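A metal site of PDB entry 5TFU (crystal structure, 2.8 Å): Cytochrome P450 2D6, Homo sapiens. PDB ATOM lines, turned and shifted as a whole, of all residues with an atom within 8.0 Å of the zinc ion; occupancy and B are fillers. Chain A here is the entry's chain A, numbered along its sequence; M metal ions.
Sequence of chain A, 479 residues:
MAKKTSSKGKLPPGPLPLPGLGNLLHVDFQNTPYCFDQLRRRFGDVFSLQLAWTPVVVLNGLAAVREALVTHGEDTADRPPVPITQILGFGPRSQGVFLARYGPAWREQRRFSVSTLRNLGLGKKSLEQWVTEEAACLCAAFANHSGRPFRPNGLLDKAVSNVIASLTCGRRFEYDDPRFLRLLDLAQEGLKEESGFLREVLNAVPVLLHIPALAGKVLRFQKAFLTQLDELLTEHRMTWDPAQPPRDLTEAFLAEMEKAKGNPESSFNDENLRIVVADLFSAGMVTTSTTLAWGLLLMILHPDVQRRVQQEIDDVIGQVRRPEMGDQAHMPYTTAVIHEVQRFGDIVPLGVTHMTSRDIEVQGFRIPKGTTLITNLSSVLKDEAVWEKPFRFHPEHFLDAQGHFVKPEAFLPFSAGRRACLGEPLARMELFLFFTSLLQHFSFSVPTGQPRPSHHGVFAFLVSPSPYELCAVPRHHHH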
ATOM      1  N   TRP A 130       3.731  19.076 -12.638  1.00  0.00           N
ATOM      2  CA  TRP A 130       5.002  18.989 -11.937  1.00  0.00           C
ATOM      3  C   TRP A 130       5.057  19.915 -10.720  1.00  0.00           C
ATOM      4  O   TRP A 130       5.671  19.580  -9.715  1.00  0.00           O
ATOM      5  CB  TRP A 130       6.169  19.301 -12.881  1.00  0.00           C
ATOM      6  CG  TRP A 130       6.581  18.148 -13.750  1.00  0.00           C
ATOM      7  CD1 TRP A 130       6.797  16.861 -13.357  1.00  0.00           C
ATOM      8  CD2 TRP A 130       6.835  18.183 -15.159  1.00  0.00           C
ATOM      9  NE1 TRP A 130       7.161  16.088 -14.437  1.00  0.00           N
ATOM     10  CE2 TRP A 130       7.196  16.876 -15.554  1.00  0.00           C
ATOM     11  CE3 TRP A 130       6.800  19.190 -16.133  1.00  0.00           C
ATOM     12  CZ2 TRP A 130       7.515  16.554 -16.872  1.00  0.00           C
ATOM     13  CZ3 TRP A 130       7.109  18.868 -17.438  1.00  0.00           C
ATOM     14  CH2 TRP A 130       7.461  17.559 -17.790  1.00  0.00           C
ATOM     15  N   ALA A 165      13.939  21.863 -13.132  1.00  0.00           N
ATOM     16  CA  ALA A 165      14.516  20.612 -13.592  1.00  0.00           C
ATOM     17  C   ALA A 165      13.464  19.761 -14.318  1.00  0.00           C
ATOM     18  O   ALA A 165      13.787  19.012 -15.227  1.00  0.00           O
ATOM     19  CB  ALA A 165      15.103  19.834 -12.432  1.00  0.00           C
ATOM     20  N   SER A 166      12.209  19.904 -13.902  1.00  0.00           N
ATOM     21  CA  SER A 166      11.115  19.191 -14.543  1.00  0.00           C
ATOM     22  C   SER A 166      10.839  19.736 -15.939  1.00  0.00           C
ATOM     23  O   SER A 166      10.315  19.028 -16.791  1.00  0.00           O
ATOM     24  CB  SER A 166       9.849  19.282 -13.682  1.00  0.00           C
ATOM     25  OG  SER A 166      10.014  18.627 -12.440  1.00  0.00           O
ATOM     26  N   LEU A 167      11.179  20.998 -16.160  1.00  0.00           N
ATOM     27  CA  LEU A 167      10.956  21.626 -17.451  1.00  0.00           C
ATOM     28  C   LEU A 167      12.177  21.481 -18.348  1.00  0.00           C
ATOM     29  O   LEU A 167      12.050  21.315 -19.563  1.00  0.00           O
ATOM     30  CB  LEU A 167      10.597  23.104 -17.283  1.00  0.00           C
ATOM     31  CG  LEU A 167       9.305  23.356 -16.513  1.00  0.00           C
ATOM     32  CD1 LEU A 167       8.885  24.808 -16.620  1.00  0.00           C
ATOM     33  CD2 LEU A 167       8.202  22.429 -16.999  1.00  0.00           C
ATOM     34  N   THR A 168      13.361  21.549 -17.751  1.00  0.00           N
ATOM     35  CA  THR A 168      14.596  21.376 -18.506  1.00  0.00           C
ATOM     36  C   THR A 168      14.904  19.900 -18.723  1.00  0.00           C
ATOM     37  O   THR A 168      14.850  19.408 -19.848  1.00  0.00           O
ATOM     38  CB  THR A 168      15.786  22.034 -17.803  1.00  0.00           C
ATOM     39  OG1 THR A 168      16.042  21.374 -16.562  1.00  0.00           O
ATOM     40  CG2 THR A 168      15.508  23.506 -17.551  1.00  0.00           C
ATOM     41  N   CYS A 169      15.223  19.196 -17.631  1.00  0.00           N
ATOM     42  CA  CYS A 169      15.675  17.812 -17.716  1.00  0.00           C
ATOM     43  C   CYS A 169      14.527  16.794 -17.607  1.00  0.00           C
ATOM     44  O   CYS A 169      14.760  15.594 -17.738  1.00  0.00           O
ATOM     45  CB  CYS A 169      16.707  17.531 -16.616  1.00  0.00           C
ATOM     46  SG  CYS A 169      18.071  18.725 -16.515  1.00  0.00           S
ATOM     47  N   GLY A 170      13.318  17.275 -17.382  1.00  0.00           N
ATOM     48  CA  GLY A 170      12.156  16.405 -17.294  1.00  0.00           C
ATOM     49  C   GLY A 170      12.175  15.473 -16.086  1.00  0.00           C
ATOM     50  O   GLY A 170      11.594  14.396 -16.110  1.00  0.00           O
ATOM     51  N   ARG A 171      12.837  15.917 -15.017  1.00  0.00           N
ATOM     52  CA  ARG A 171      12.956  15.109 -13.810  1.00  0.00           C
ATOM     53  C   ARG A 171      13.017  15.971 -12.558  1.00  0.00           C
ATOM     54  O   ARG A 171      13.254  17.173 -12.629  1.00  0.00           O
ATOM     55  CB  ARG A 171      14.204  14.226 -13.873  1.00  0.00           C
ATOM     56  CG  ARG A 171      15.497  15.009 -13.722  1.00  0.00           C
ATOM     57  CD  ARG A 171      16.641  14.122 -13.282  1.00  0.00           C
ATOM     58  NE  ARG A 171      16.442  13.595 -11.945  1.00  0.00           N
ATOM     59  CZ  ARG A 171      17.262  12.748 -11.332  1.00  0.00           C
ATOM     60  NH1 ARG A 171      18.360  12.335 -11.958  1.00  0.00           N
ATOM     61  NH2 ARG A 171      17.003  12.323 -10.113  1.00  0.00           N
ATOM     62  N   HIS A 236      21.081  12.859 -19.275  1.00  0.00           N
ATOM     63  CA  HIS A 236      19.786  13.107 -19.898  1.00  0.00           C
ATOM     64  C   HIS A 236      19.792  12.777 -21.391  1.00  0.00           C
ATOM     65  O   HIS A 236      18.799  12.286 -21.933  1.00  0.00           O
ATOM     66  CB  HIS A 236      19.369  14.558 -19.694  1.00  0.00           C
ATOM     67  CG  HIS A 236      17.990  14.862 -20.168  1.00  0.00           C
ATOM     68  ND1 HIS A 236      17.616  16.099 -20.651  1.00  0.00           N
ATOM     69  CD2 HIS A 236      16.877  14.089 -20.229  1.00  0.00           C
ATOM     70  CE1 HIS A 236      16.340  16.071 -20.999  1.00  0.00           C
ATOM     71  NE2 HIS A 236      15.874  14.869 -20.748  1.00  0.00           N
ATOM     72  N   ARG A 237      20.916  13.041 -22.052  1.00  0.00           N
ATOM     73  CA  ARG A 237      21.049  12.766 -23.476  1.00  0.00           C
ATOM     74  C   ARG A 237      20.957  11.266 -23.745  1.00  0.00           C
ATOM     75  O   ARG A 237      20.534  10.852 -24.824  1.00  0.00           O
ATOM     76  CB  ARG A 237      22.378  13.312 -24.004  1.00  0.00           C
ATOM     77  CG  ARG A 237      22.480  13.346 -25.526  1.00  0.00           C
ATOM     78  CD  ARG A 237      23.886  13.729 -25.970  1.00  0.00           C
ATOM     79  NE  ARG A 237      24.313  15.011 -25.414  1.00  0.00           N
ATOM     80  CZ  ARG A 237      24.267  16.166 -26.070  1.00  0.00           C
ATOM     81  NH1 ARG A 237      23.810  16.197 -27.310  1.00  0.00           N
ATOM     82  NH2 ARG A 237      24.670  17.276 -25.485  1.00  0.00           N
ATOM     83  N   THR A 239      19.032   9.077 -22.018  1.00  0.00           N
ATOM     84  CA  THR A 239      17.674   8.585 -21.814  1.00  0.00           C
ATOM     85  C   THR A 239      16.673   9.189 -22.793  1.00  0.00           C
ATOM     86  O   THR A 239      15.505   8.794 -22.825  1.00  0.00           O
ATOM     87  CB  THR A 239      17.180   8.862 -20.380  1.00  0.00           C
ATOM     88  OG1 THR A 239      17.198  10.284 -20.138  1.00  0.00           O
ATOM     89  CG2 THR A 239      18.079   8.171 -19.365  1.00  0.00           C
ATOM     90  N   TRP A 240      17.126  10.157 -23.574  1.00  0.00           N
ATOM     91  CA  TRP A 240      16.246  10.864 -24.505  1.00  0.00           C
ATOM     92  C   TRP A 240      15.818   9.967 -25.669  1.00  0.00           C
ATOM     93  O   TRP A 240      16.650   9.379 -26.357  1.00  0.00           O
ATOM     94  CB  TRP A 240      16.936  12.124 -25.034  1.00  0.00           C
ATOM     95  CG  TRP A 240      16.262  12.745 -26.214  1.00  0.00           C
ATOM     96  CD1 TRP A 240      14.937  13.038 -26.349  1.00  0.00           C
ATOM     97  CD2 TRP A 240      16.893  13.169 -27.429  1.00  0.00           C
ATOM     98  NE1 TRP A 240      14.701  13.608 -27.569  1.00  0.00           N
ATOM     99  CE2 TRP A 240      15.881  13.700 -28.253  1.00  0.00           C
ATOM    100  CE3 TRP A 240      18.207  13.146 -27.902  1.00  0.00           C
ATOM    101  CZ2 TRP A 240      16.141  14.211 -29.527  1.00  0.00           C
ATOM    102  CZ3 TRP A 240      18.467  13.656 -29.162  1.00  0.00           C
ATOM    103  CH2 TRP A 240      17.436  14.171 -29.958  1.00  0.00           C
ATOM    104  N   ASP A 241      14.509   9.872 -25.868  1.00  0.00           N
ATOM    105  CA  ASP A 241      13.947   9.118 -26.988  1.00  0.00           C
ATOM    106  C   ASP A 241      13.444  10.067 -28.071  1.00  0.00           C
ATOM    107  O   ASP A 241      12.383  10.676 -27.918  1.00  0.00           O
ATOM    108  CB  ASP A 241      12.823   8.200 -26.511  1.00  0.00           C
ATOM    109  CG  ASP A 241      12.372   7.223 -27.583  1.00  0.00           C
ATOM    110  OD1 ASP A 241      11.286   6.622 -27.432  1.00  0.00           O
ATOM    111  OD2 ASP A 241      13.102   7.053 -28.580  1.00  0.00           O
ATOM    112  N   PRO A 245       7.679  12.712 -29.007  1.00  0.00           N
ATOM    113  CA  PRO A 245       7.694  14.169 -28.828  1.00  0.00           C
ATOM    114  C   PRO A 245       8.433  14.556 -27.555  1.00  0.00           C
ATOM    115  O   PRO A 245       8.299  13.852 -26.558  1.00  0.00           O
ATOM    116  CB  PRO A 245       6.214  14.533 -28.749  1.00  0.00           C
ATOM    117  CG  PRO A 245       5.517  13.431 -29.465  1.00  0.00           C
ATOM    118  CD  PRO A 245       6.311  12.192 -29.171  1.00  0.00           C
ATOM    119  N   PRO A 246       9.203  15.652 -27.590  1.00  0.00           N
ATOM    120  CA  PRO A 246      10.016  16.095 -26.451  1.00  0.00           C
ATOM    121  C   PRO A 246       9.213  16.215 -25.156  1.00  0.00           C
ATOM    122  O   PRO A 246       8.185  16.892 -25.138  1.00  0.00           O
ATOM    123  CB  PRO A 246      10.545  17.460 -26.900  1.00  0.00           C
ATOM    124  CG  PRO A 246      10.548  17.386 -28.378  1.00  0.00           C
ATOM    125  CD  PRO A 246       9.357  16.550 -28.750  1.00  0.00           C
ATOM    126  N   ARG A 247       9.678  15.554 -24.108  1.00  0.00           N
ATOM    127  CA  ARG A 247       9.029  15.645 -22.800  1.00  0.00           C
ATOM    128  C   ARG A 247       9.386  16.942 -22.095  1.00  0.00           C
ATOM    129  O   ARG A 247       8.657  17.403 -21.217  1.00  0.00           O
ATOM    130  CB  ARG A 247       9.421  14.473 -21.901  1.00  0.00           C
ATOM    131  CG  ARG A 247       8.779  13.149 -22.264  1.00  0.00           C
ATOM    132  CD  ARG A 247       8.768  12.222 -21.049  1.00  0.00           C
ATOM    133  NE  ARG A 247       9.823  12.539 -20.090  1.00  0.00           N
ATOM    134  CZ  ARG A 247       9.613  13.071 -18.885  1.00  0.00           C
ATOM    135  NH1 ARG A 247       8.377  13.336 -18.491  1.00  0.00           N
ATOM    136  NH2 ARG A 247      10.641  13.330 -18.082  1.00  0.00           N
ATOM    137  N   ASP A 248      10.511  17.532 -22.473  1.00  0.00           N
ATOM    138  CA  ASP A 248      11.040  18.703 -21.784  1.00  0.00           C
ATOM    139  C   ASP A 248      11.807  19.630 -22.724  1.00  0.00           C
ATOM    140  O   ASP A 248      11.996  19.317 -23.893  1.00  0.00           O
ATOM    141  CB  ASP A 248      11.927  18.259 -20.619  1.00  0.00           C
ATOM    142  CG  ASP A 248      12.927  17.204 -21.027  1.00  0.00           C
ATOM    143  OD1 ASP A 248      13.883  17.538 -21.757  1.00  0.00           O
ATOM    144  OD2 ASP A 248      12.771  16.038 -20.617  1.00  0.00           O
ATOM    145  N   LEU A 249      12.247  20.765 -22.189  1.00  0.00           N
ATOM    146  CA  LEU A 249      12.884  21.800 -22.979  1.00  0.00           C
ATOM    147  C   LEU A 249      14.208  21.337 -23.580  1.00  0.00           C
ATOM    148  O   LEU A 249      14.555  21.692 -24.707  1.00  0.00           O
ATOM    149  CB  LEU A 249      13.115  23.056 -22.131  1.00  0.00           C
ATOM    150  CG  LEU A 249      13.684  24.297 -22.821  1.00  0.00           C
ATOM    151  CD1 LEU A 249      12.978  25.543 -22.310  1.00  0.00           C
ATOM    152  CD2 LEU A 249      15.182  24.410 -22.581  1.00  0.00           C
ATOM    153  N   THR A 250      14.954  20.540 -22.824  1.00  0.00           N
ATOM    154  CA  THR A 250      16.243  20.031 -23.284  1.00  0.00           C
ATOM    155  C   THR A 250      16.049  19.099 -24.478  1.00  0.00           C
ATOM    156  O   THR A 250      16.784  19.185 -25.461  1.00  0.00           O
ATOM    157  CB  THR A 250      16.998  19.290 -22.161  1.00  0.00           C
ATOM    158  OG1 THR A 250      17.254  20.199 -21.080  1.00  0.00           O
ATOM    159  CG2 THR A 250      18.312  18.727 -22.662  1.00  0.00           C
ATOM    160  N   GLU A 251      15.047  18.229 -24.391  1.00  0.00           N
ATOM    161  CA  GLU A 251      14.719  17.334 -25.492  1.00  0.00           C
ATOM    162  C   GLU A 251      14.291  18.120 -26.718  1.00  0.00           C
ATOM    163  O   GLU A 251      14.598  17.740 -27.853  1.00  0.00           O
ATOM    164  CB  GLU A 251      13.632  16.342 -25.080  1.00  0.00           C
ATOM    165  CG  GLU A 251      14.067  15.358 -24.011  1.00  0.00           C
ATOM    166  CD  GLU A 251      12.991  14.347 -23.662  1.00  0.00           C
ATOM    167  OE1 GLU A 251      12.012  14.220 -24.423  1.00  0.00           O
ATOM    168  OE2 GLU A 251      13.126  13.675 -22.618  1.00  0.00           O
ATOM    169  N   ALA A 252      13.576  19.224 -26.490  1.00  0.00           N
ATOM    170  CA  ALA A 252      13.161  20.104 -27.580  1.00  0.00           C
ATOM    171  C   ALA A 252      14.373  20.823 -28.164  1.00  0.00           C
ATOM    172  O   ALA A 252      14.415  21.100 -29.366  1.00  0.00           O
ATOM    173  CB  ALA A 252      12.136  21.106 -27.081  1.00  0.00           C
ATOM    174  N   LEU A 254      17.507  19.558 -28.070  1.00  0.00           N
ATOM    175  CA  LEU A 254      18.263  18.509 -28.744  1.00  0.00           C
ATOM    176  C   LEU A 254      17.686  18.201 -30.124  1.00  0.00           C
ATOM    177  O   LEU A 254      18.422  17.968 -31.087  1.00  0.00           O
ATOM    178  CB  LEU A 254      18.292  17.231 -27.897  1.00  0.00           C
ATOM    179  CG  LEU A 254      19.035  17.270 -26.561  1.00  0.00           C
ATOM    180  CD1 LEU A 254      18.792  15.988 -25.775  1.00  0.00           C
ATOM    181  CD2 LEU A 254      20.528  17.490 -26.766  1.00  0.00           C
HETATM  182 ZN    ZN M   1      13.951  14.460 -21.012  1.00  0.00          ZN
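The side-chain carboxylate of Glu 251 sits at hydrogen-bond distance from the backbone NH of Arg 247 (2.7 Å).
A ring nitrogen (NE2) of His 236 lies close to the backbone carbonyl oxygen (O) of Cys 169, 3.3 Å away.
O of His 236 sits at hydrogen-bond distance from OG1 of Thr 239 (3.1 Å).
The side-chain carboxylate (OD1) of Asp 248 sits close to the backbone NH (N) of Thr 250 (3.4 Å).
OG1 of Thr 168 sits at hydrogen-bond distance from SG of Cys 169, 3.3 Å away.
The zinc ion is bound by OE2 of Glu 251 (2.0 Å), NE2 of His 236 (2.0 Å) and OD2 of Asp 248 (2.0 Å).
Residues that only touch the zinc ion: Cys 169 (3.6 Å).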
